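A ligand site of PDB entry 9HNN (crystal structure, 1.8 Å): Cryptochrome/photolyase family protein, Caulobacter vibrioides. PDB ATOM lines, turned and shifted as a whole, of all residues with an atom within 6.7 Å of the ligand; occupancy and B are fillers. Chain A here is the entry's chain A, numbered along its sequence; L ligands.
The side-chain sulfur (SG) of Cys 440 binds an iron atom (FE4) of the ligand, at 2.2 Å. The side-chain sulfur (SG) of Cys 437 is bound to an iron atom (FE1) of the ligand (2.3 Å). FE2 of the ligand is bound by SG of Cys 453, at 2.3 Å. SG of Cys 349 binds FE3 of the ligand (2.3 Å).
Met 347 touches the ligand (CB to S1, 3.2 Å). Gly 427 touches the ligand. Ile 430 touches the ligand. Tyr 436 touches the ligand (CB to S2, 3.6 Å). Val 444 touches the ligand. Phe 455 touches the ligand. Hydrophobic or aromatic side chains within 4 Å of the ligand: Met 347, Ile 430, Tyr 436, Val 444 and Phe 455. Within 4 Å of the ligand: Met 347, Cys 349, Gly 427, Ile 430, Tyr 436, Cys 437, Cys 440, Val 444, Cys 453 and Phe 455.
SG of Cys 440 sits close to N of Tyr 442 (3.8 Å). The side-chain sulfur of Cys 440 lies close to the backbone NH of Ala 348, at 3.5 Å. The backbone carbonyl oxygen of Asp 346 sits close to the side-chain sulfur of Cys 440 (3.6 Å). SG of Cys 453 lies close to N of Phe 455 (3.4 Å). The backbone NH (N) of Cys 453 lies within hydrogen-bond range of the backbone carbonyl oxygen (O) of Asp 443, at 3.1 Å. The backbone NH (N) of Tyr 436 is in hydrogen-bond range of the side-chain hydroxyl (OG) of Ser 434, 3.3 Å away. The side-chain hydroxyl of Ser 434 is in hydrogen-bond range of the backbone carbonyl oxygen of Ile 430, at 2.5 Å. O of Val 444 sits at hydrogen-bond distance from ND2 of Asn 456 (3.1 Å).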
ATOM      1  N   ASP A 346     -22.576  -2.549  22.680  1.00  0.00           N
ATOM      2  CA  ASP A 346     -23.274  -3.485  21.803  1.00  0.00           C
ATOM      3  C   ASP A 346     -22.521  -4.794  21.581  1.00  0.00           C
ATOM      4  O   ASP A 346     -23.068  -5.672  20.909  1.00  0.00           O
ATOM      5  CB  ASP A 346     -23.583  -2.850  20.450  1.00  0.00           C
ATOM      6  CG  ASP A 346     -24.645  -1.762  20.515  1.00  0.00           C
ATOM      7  OD1 ASP A 346     -25.686  -1.969  21.187  1.00  0.00           O
ATOM      8  OD2 ASP A 346     -24.465  -0.715  19.869  1.00  0.00           O
ATOM      9  N   MET A 347     -21.304  -4.984  22.100  1.00  0.00           N
ATOM     10  CA  MET A 347     -20.778  -6.332  22.021  1.00  0.00           C
ATOM     11  C   MET A 347     -21.380  -7.211  23.134  1.00  0.00           C
ATOM     12  O   MET A 347     -21.116  -7.018  24.330  1.00  0.00           O
ATOM     13  CB  MET A 347     -19.250  -6.414  21.918  1.00  0.00           C
ATOM     14  CG  MET A 347     -18.443  -5.252  21.321  1.00  0.00           C
ATOM     15  SD  MET A 347     -16.669  -5.282  21.690  1.00  0.00           S
ATOM     16  CE  MET A 347     -16.548  -4.114  23.047  1.00  0.00           C
ATOM     17  N   ALA A 348     -22.203  -8.176  22.694  1.00  0.00           N
ATOM     18  CA  ALA A 348     -23.028  -8.954  23.602  1.00  0.00           C
ATOM     19  C   ALA A 348     -22.202  -9.779  24.583  1.00  0.00           C
ATOM     20  O   ALA A 348     -22.671 -10.051  25.690  1.00  0.00           O
ATOM     21  CB  ALA A 348     -23.940  -9.890  22.805  1.00  0.00           C
ATOM     22  N   CYS A 349     -20.996 -10.203  24.174  1.00  0.00           N
ATOM     23  CA  CYS A 349     -20.152 -11.033  25.024  1.00  0.00           C
ATOM     24  C   CYS A 349     -19.544 -10.215  26.158  1.00  0.00           C
ATOM     25  O   CYS A 349     -19.560 -10.631  27.326  1.00  0.00           O
ATOM     26  CB  CYS A 349     -19.038 -11.685  24.206  1.00  0.00           C
ATOM     27  SG  CYS A 349     -18.115 -10.564  23.101  1.00  0.00           S
ATOM     28  N   VAL A 350     -19.008  -9.054  25.824  1.00  0.00           N
ATOM     29  CA  VAL A 350     -18.494  -8.140  26.843  1.00  0.00           C
ATOM     30  C   VAL A 350     -19.613  -7.719  27.795  1.00  0.00           C
ATOM     31  O   VAL A 350     -19.475  -7.783  29.021  1.00  0.00           O
ATOM     32  CB  VAL A 350     -17.825  -6.925  26.180  1.00  0.00           C
ATOM     33  CG1 VAL A 350     -17.240  -5.981  27.223  1.00  0.00           C
ATOM     34  CG2 VAL A 350     -16.761  -7.391  25.224  1.00  0.00           C
ATOM     35  N   VAL A 371     -12.593 -13.036  27.029  1.00  0.00           N
ATOM     36  CA  VAL A 371     -13.483 -11.918  26.686  1.00  0.00           C
ATOM     37  C   VAL A 371     -12.854 -10.619  27.190  1.00  0.00           C
ATOM     38  O   VAL A 371     -12.189  -9.916  26.421  1.00  0.00           O
ATOM     39  CB  VAL A 371     -14.890 -12.138  27.269  1.00  0.00           C
ATOM     40  CG1 VAL A 371     -15.808 -10.997  26.926  1.00  0.00           C
ATOM     41  CG2 VAL A 371     -15.476 -13.438  26.742  1.00  0.00           C
ATOM     42  N   SER A 426      -9.565 -13.945  17.959  1.00  0.00           N
ATOM     43  CA  SER A 426     -10.551 -13.185  17.200  1.00  0.00           C
ATOM     44  C   SER A 426     -11.968 -13.568  17.649  1.00  0.00           C
ATOM     45  O   SER A 426     -12.167 -14.394  18.545  1.00  0.00           O
ATOM     46  CB  SER A 426     -10.383 -13.429  15.707  1.00  0.00           C
ATOM     47  OG  SER A 426     -10.844 -14.710  15.323  1.00  0.00           O
ATOM     48  N   GLY A 427     -12.970 -12.976  17.010  1.00  0.00           N
ATOM     49  CA  GLY A 427     -14.345 -13.307  17.349  1.00  0.00           C
ATOM     50  C   GLY A 427     -14.712 -14.749  17.031  1.00  0.00           C
ATOM     51  O   GLY A 427     -15.684 -15.263  17.603  1.00  0.00           O
ATOM     52  N   ALA A 428     -13.966 -15.408  16.155  1.00  0.00           N
ATOM     53  CA  ALA A 428     -14.310 -16.759  15.750  1.00  0.00           C
ATOM     54  C   ALA A 428     -14.199 -17.734  16.919  1.00  0.00           C
ATOM     55  O   ALA A 428     -14.970 -18.694  16.987  1.00  0.00           O
ATOM     56  CB  ALA A 428     -13.421 -17.210  14.596  1.00  0.00           C
ATOM     57  N   ILE A 430     -14.800 -16.998  20.191  1.00  0.00           N
ATOM     58  CA  ILE A 430     -15.963 -16.741  21.035  1.00  0.00           C
ATOM     59  C   ILE A 430     -17.231 -17.310  20.393  1.00  0.00           C
ATOM     60  O   ILE A 430     -18.110 -17.840  21.089  1.00  0.00           O
ATOM     61  CB  ILE A 430     -16.094 -15.237  21.326  1.00  0.00           C
ATOM     62  CG1 ILE A 430     -14.932 -14.763  22.215  1.00  0.00           C
ATOM     63  CG2 ILE A 430     -17.449 -14.888  21.937  1.00  0.00           C
ATOM     64  CD1 ILE A 430     -14.853 -13.263  22.384  1.00  0.00           C
ATOM     65  N   ASP A 431     -17.341 -17.206  19.074  1.00  0.00           N
ATOM     66  CA  ASP A 431     -18.482 -17.799  18.377  1.00  0.00           C
ATOM     67  C   ASP A 431     -18.485 -19.321  18.522  1.00  0.00           C
ATOM     68  O   ASP A 431     -19.538 -19.936  18.713  1.00  0.00           O
ATOM     69  CB  ASP A 431     -18.463 -17.372  16.904  1.00  0.00           C
ATOM     70  CG  ASP A 431     -19.593 -17.993  16.104  1.00  0.00           C
ATOM     71  OD1 ASP A 431     -20.757 -17.944  16.554  1.00  0.00           O
ATOM     72  OD2 ASP A 431     -19.310 -18.526  15.010  1.00  0.00           O
ATOM     73  N   SER A 434     -19.639 -20.360  22.324  1.00  0.00           N
ATOM     74  CA  SER A 434     -20.737 -19.631  22.941  1.00  0.00           C
ATOM     75  C   SER A 434     -21.927 -19.536  21.996  1.00  0.00           C
ATOM     76  O   SER A 434     -21.847 -19.897  20.822  1.00  0.00           O
ATOM     77  CB  SER A 434     -20.294 -18.218  23.338  1.00  0.00           C
ATOM     78  OG  SER A 434     -20.274 -17.391  22.201  1.00  0.00           O
ATOM     79  N   TYR A 436     -23.355 -16.444  21.758  1.00  0.00           N
ATOM     80  CA  TYR A 436     -23.426 -14.992  21.868  1.00  0.00           C
ATOM     81  C   TYR A 436     -23.681 -14.323  20.526  1.00  0.00           C
ATOM     82  O   TYR A 436     -24.518 -13.426  20.419  1.00  0.00           O
ATOM     83  CB  TYR A 436     -22.099 -14.457  22.423  1.00  0.00           C
ATOM     84  CG  TYR A 436     -21.943 -14.488  23.911  1.00  0.00           C
ATOM     85  CD1 TYR A 436     -22.996 -14.159  24.749  1.00  0.00           C
ATOM     86  CD2 TYR A 436     -20.729 -14.835  24.470  1.00  0.00           C
ATOM     87  CE1 TYR A 436     -22.834 -14.176  26.138  1.00  0.00           C
ATOM     88  CE2 TYR A 436     -20.557 -14.862  25.849  1.00  0.00           C
ATOM     89  CZ  TYR A 436     -21.608 -14.522  26.679  1.00  0.00           C
ATOM     90  OH  TYR A 436     -21.424 -14.549  28.049  1.00  0.00           O
ATOM     91  N   CYS A 437     -22.925 -14.719  19.501  1.00  0.00           N
ATOM     92  CA  CYS A 437     -22.867 -13.897  18.298  1.00  0.00           C
ATOM     93  C   CYS A 437     -24.194 -13.887  17.546  1.00  0.00           C
ATOM     94  O   CYS A 437     -24.494 -12.891  16.871  1.00  0.00           O
ATOM     95  CB  CYS A 437     -21.718 -14.404  17.432  1.00  0.00           C
ATOM     96  SG  CYS A 437     -20.180 -14.553  18.382  1.00  0.00           S
ATOM     97  N   LYS A 438     -25.014 -14.940  17.666  1.00  0.00           N
ATOM     98  CA  LYS A 438     -26.299 -14.932  16.972  1.00  0.00           C
ATOM     99  C   LYS A 438     -27.183 -13.775  17.430  1.00  0.00           C
ATOM    100  O   LYS A 438     -27.990 -13.253  16.649  1.00  0.00           O
ATOM    101  CB  LYS A 438     -27.069 -16.246  17.179  1.00  0.00           C
ATOM    102  CG  LYS A 438     -27.133 -16.737  18.626  1.00  0.00           C
ATOM    103  CD  LYS A 438     -26.956 -18.249  18.729  1.00  0.00           C
ATOM    104  CE  LYS A 438     -28.014 -19.012  17.952  1.00  0.00           C
ATOM    105  NZ  LYS A 438     -29.366 -18.843  18.541  1.00  0.00           N
ATOM    106  N   GLY A 439     -27.055 -13.365  18.684  1.00  0.00           N
ATOM    107  CA  GLY A 439     -27.814 -12.252  19.227  1.00  0.00           C
ATOM    108  C   GLY A 439     -27.095 -10.924  19.177  1.00  0.00           C
ATOM    109  O   GLY A 439     -27.669  -9.907  19.553  1.00  0.00           O
ATOM    110  N   CYS A 440     -25.843 -10.921  18.726  1.00  0.00           N
ATOM    111  CA  CYS A 440     -25.054  -9.710  18.662  1.00  0.00           C
ATOM    112  C   CYS A 440     -25.408  -8.903  17.415  1.00  0.00           C
ATOM    113  O   CYS A 440     -25.629  -9.470  16.331  1.00  0.00           O
ATOM    114  CB  CYS A 440     -23.569 -10.065  18.651  1.00  0.00           C
ATOM    115  SG  CYS A 440     -22.506  -8.779  19.239  1.00  0.00           S
ATOM    116  N   ARG A 441     -25.449  -7.581  17.564  1.00  0.00           N
ATOM    117  CA  ARG A 441     -25.677  -6.727  16.403  1.00  0.00           C
ATOM    118  C   ARG A 441     -24.490  -6.720  15.464  1.00  0.00           C
ATOM    119  O   ARG A 441     -24.628  -6.321  14.300  1.00  0.00           O
ATOM    120  CB  ARG A 441     -26.000  -5.297  16.848  1.00  0.00           C
ATOM    121  CG  ARG A 441     -24.779  -4.456  17.171  1.00  0.00           C
ATOM    122  CD  ARG A 441     -25.006  -3.003  16.798  1.00  0.00           C
ATOM    123  NE  ARG A 441     -24.741  -2.740  15.394  1.00  0.00           N
ATOM    124  CZ  ARG A 441     -23.635  -2.155  14.943  1.00  0.00           C
ATOM    125  NH1 ARG A 441     -22.669  -1.784  15.759  1.00  0.00           N
ATOM    126  NH2 ARG A 441     -23.509  -1.923  13.635  1.00  0.00           N
ATOM    127  N   TYR A 442     -23.312  -7.142  15.927  1.00  0.00           N
ATOM    128  CA  TYR A 442     -22.146  -7.225  15.065  1.00  0.00           C
ATOM    129  C   TYR A 442     -22.159  -8.535  14.287  1.00  0.00           C
ATOM    130  O   TYR A 442     -22.750  -9.532  14.714  1.00  0.00           O
ATOM    131  CB  TYR A 442     -20.857  -7.139  15.884  1.00  0.00           C
ATOM    132  CG  TYR A 442     -20.654  -5.803  16.562  1.00  0.00           C
ATOM    133  CD1 TYR A 442     -20.398  -4.658  15.817  1.00  0.00           C
ATOM    134  CD2 TYR A 442     -20.729  -5.685  17.941  1.00  0.00           C
ATOM    135  CE1 TYR A 442     -20.218  -3.441  16.415  1.00  0.00           C
ATOM    136  CE2 TYR A 442     -20.550  -4.450  18.561  1.00  0.00           C
ATOM    137  CZ  TYR A 442     -20.293  -3.331  17.783  1.00  0.00           C
ATOM    138  OH  TYR A 442     -20.121  -2.111  18.370  1.00  0.00           O
ATOM    139  N   ASP A 443     -21.463  -8.524  13.151  1.00  0.00           N
ATOM    140  CA  ASP A 443     -21.300  -9.701  12.315  1.00  0.00           C
ATOM    141  C   ASP A 443     -19.915 -10.272  12.547  1.00  0.00           C
ATOM    142  O   ASP A 443     -18.896  -9.621  12.264  1.00  0.00           O
ATOM    143  CB  ASP A 443     -21.525  -9.370  10.834  1.00  0.00           C
ATOM    144  CG  ASP A 443     -21.776 -10.617   9.987  1.00  0.00           C
ATOM    145  OD1 ASP A 443     -21.041 -11.606  10.169  1.00  0.00           O
ATOM    146  OD2 ASP A 443     -22.705 -10.612   9.143  1.00  0.00           O
ATOM    147  N   VAL A 444     -19.877 -11.497  13.082  1.00  0.00           N
ATOM    148  CA  VAL A 444     -18.630 -12.191  13.410  1.00  0.00           C
ATOM    149  C   VAL A 444     -17.920 -12.714  12.169  1.00  0.00           C
ATOM    150  O   VAL A 444     -16.777 -13.181  12.254  1.00  0.00           O
ATOM    151  CB  VAL A 444     -18.930 -13.325  14.405  1.00  0.00           C
ATOM    152  CG1 VAL A 444     -19.477 -14.539  13.670  1.00  0.00           C
ATOM    153  CG2 VAL A 444     -17.695 -13.683  15.241  1.00  0.00           C
ATOM    154  N   LYS A 445     -18.576 -12.642  11.017  1.00  0.00           N
ATOM    155  CA  LYS A 445     -17.959 -13.078   9.793  1.00  0.00           C
ATOM    156  C   LYS A 445     -17.197 -11.960   9.112  1.00  0.00           C
ATOM    157  O   LYS A 445     -16.346 -12.226   8.250  1.00  0.00           O
ATOM    158  CB  LYS A 445     -19.022 -13.644   8.846  1.00  0.00           C
ATOM    159  CG  LYS A 445     -19.679 -14.895   9.394  1.00  0.00           C
ATOM    160  CD  LYS A 445     -19.055 -16.145   8.834  1.00  0.00           C
ATOM    161  CE  LYS A 445     -20.125 -17.027   8.193  1.00  0.00           C
ATOM    162  N   ALA A 452     -18.991  -4.859  11.715  1.00  0.00           N
ATOM    163  CA  ALA A 452     -18.029  -5.928  11.952  1.00  0.00           C
ATOM    164  C   ALA A 452     -17.758  -6.111  13.438  1.00  0.00           C
ATOM    165  O   ALA A 452     -17.839  -5.169  14.227  1.00  0.00           O
ATOM    166  CB  ALA A 452     -16.707  -5.649  11.221  1.00  0.00           C
ATOM    167  N   CYS A 453     -17.434  -7.341  13.813  1.00  0.00           N
ATOM    168  CA  CYS A 453     -17.122  -7.646  15.198  1.00  0.00           C
ATOM    169  C   CYS A 453     -15.763  -7.057  15.561  1.00  0.00           C
ATOM    170  O   CYS A 453     -14.776  -7.331  14.882  1.00  0.00           O
ATOM    171  CB  CYS A 453     -17.106  -9.153  15.440  1.00  0.00           C
ATOM    172  SG  CYS A 453     -16.283  -9.599  16.978  1.00  0.00           S
ATOM    173  N   PRO A 454     -15.676  -6.252  16.634  1.00  0.00           N
ATOM    174  CA  PRO A 454     -14.417  -5.553  16.934  1.00  0.00           C
ATOM    175  C   PRO A 454     -13.251  -6.475  17.210  1.00  0.00           C
ATOM    176  O   PRO A 454     -12.101  -6.037  17.125  1.00  0.00           O
ATOM    177  CB  PRO A 454     -14.774  -4.708  18.167  1.00  0.00           C
ATOM    178  CG  PRO A 454     -16.251  -4.501  18.070  1.00  0.00           C
ATOM    179  CD  PRO A 454     -16.799  -5.761  17.451  1.00  0.00           C
ATOM    180  N   PHE A 455     -13.504  -7.735  17.544  1.00  0.00           N
ATOM    181  CA  PHE A 455     -12.408  -8.650  17.892  1.00  0.00           C
ATOM    182  C   PHE A 455     -11.591  -9.024  16.665  1.00  0.00           C
ATOM    183  O   PHE A 455     -10.411  -9.380  16.801  1.00  0.00           O
ATOM    184  CB  PHE A 455     -12.960  -9.916  18.546  1.00  0.00           C
ATOM    185  CG  PHE A 455     -13.324  -9.740  20.001  1.00  0.00           C
ATOM    186  CD1 PHE A 455     -12.380  -9.897  20.982  1.00  0.00           C
ATOM    187  CD2 PHE A 455     -14.623  -9.454  20.379  1.00  0.00           C
ATOM    188  CE1 PHE A 455     -12.710  -9.748  22.316  1.00  0.00           C
ATOM    189  CE2 PHE A 455     -14.965  -9.315  21.720  1.00  0.00           C
ATOM    190  CZ  PHE A 455     -14.008  -9.461  22.684  1.00  0.00           C
ATOM    191  N   ASN A 456     -12.193  -8.972  15.479  1.00  0.00           N
ATOM    192  CA  ASN A 456     -11.519  -9.480  14.295  1.00  0.00           C
ATOM    193  C   ASN A 456     -10.445  -8.511  13.806  1.00  0.00           C
ATOM    194  O   ASN A 456      -9.287  -8.902  13.628  1.00  0.00           O
ATOM    195  CB  ASN A 456     -12.544  -9.806  13.201  1.00  0.00           C
ATOM    196  CG  ASN A 456     -13.503 -10.919  13.618  1.00  0.00           C
ATOM    197  OD1 ASN A 456     -13.165 -11.748  14.453  1.00  0.00           O
ATOM    198  ND2 ASN A 456     -14.705 -10.944  13.034  1.00  0.00           N
HETATM  199 FE1  LIG L   1     -19.582 -12.443  18.911  1.00  0.00          FE
HETATM  200 FE2  LIG L   1     -18.008 -10.269  18.312  1.00  0.00          FE
HETATM  201 FE3  LIG L   1     -18.634 -10.843  20.887  1.00  0.00          FE
HETATM  202 FE4  LIG L   1     -20.568  -9.885  19.142  1.00  0.00          FE
HETATM  203  S1  LIG L   1     -18.732  -8.802  19.853  1.00  0.00           S
HETATM  204  S2  LIG L   1     -20.764 -11.629  20.647  1.00  0.00           S
HETATM  205  S3  LIG L   1     -19.902 -10.889  17.232  1.00  0.00           S
HETATM  206  S4  LIG L   1     -17.406 -12.139  19.516  1.00  0.00           S
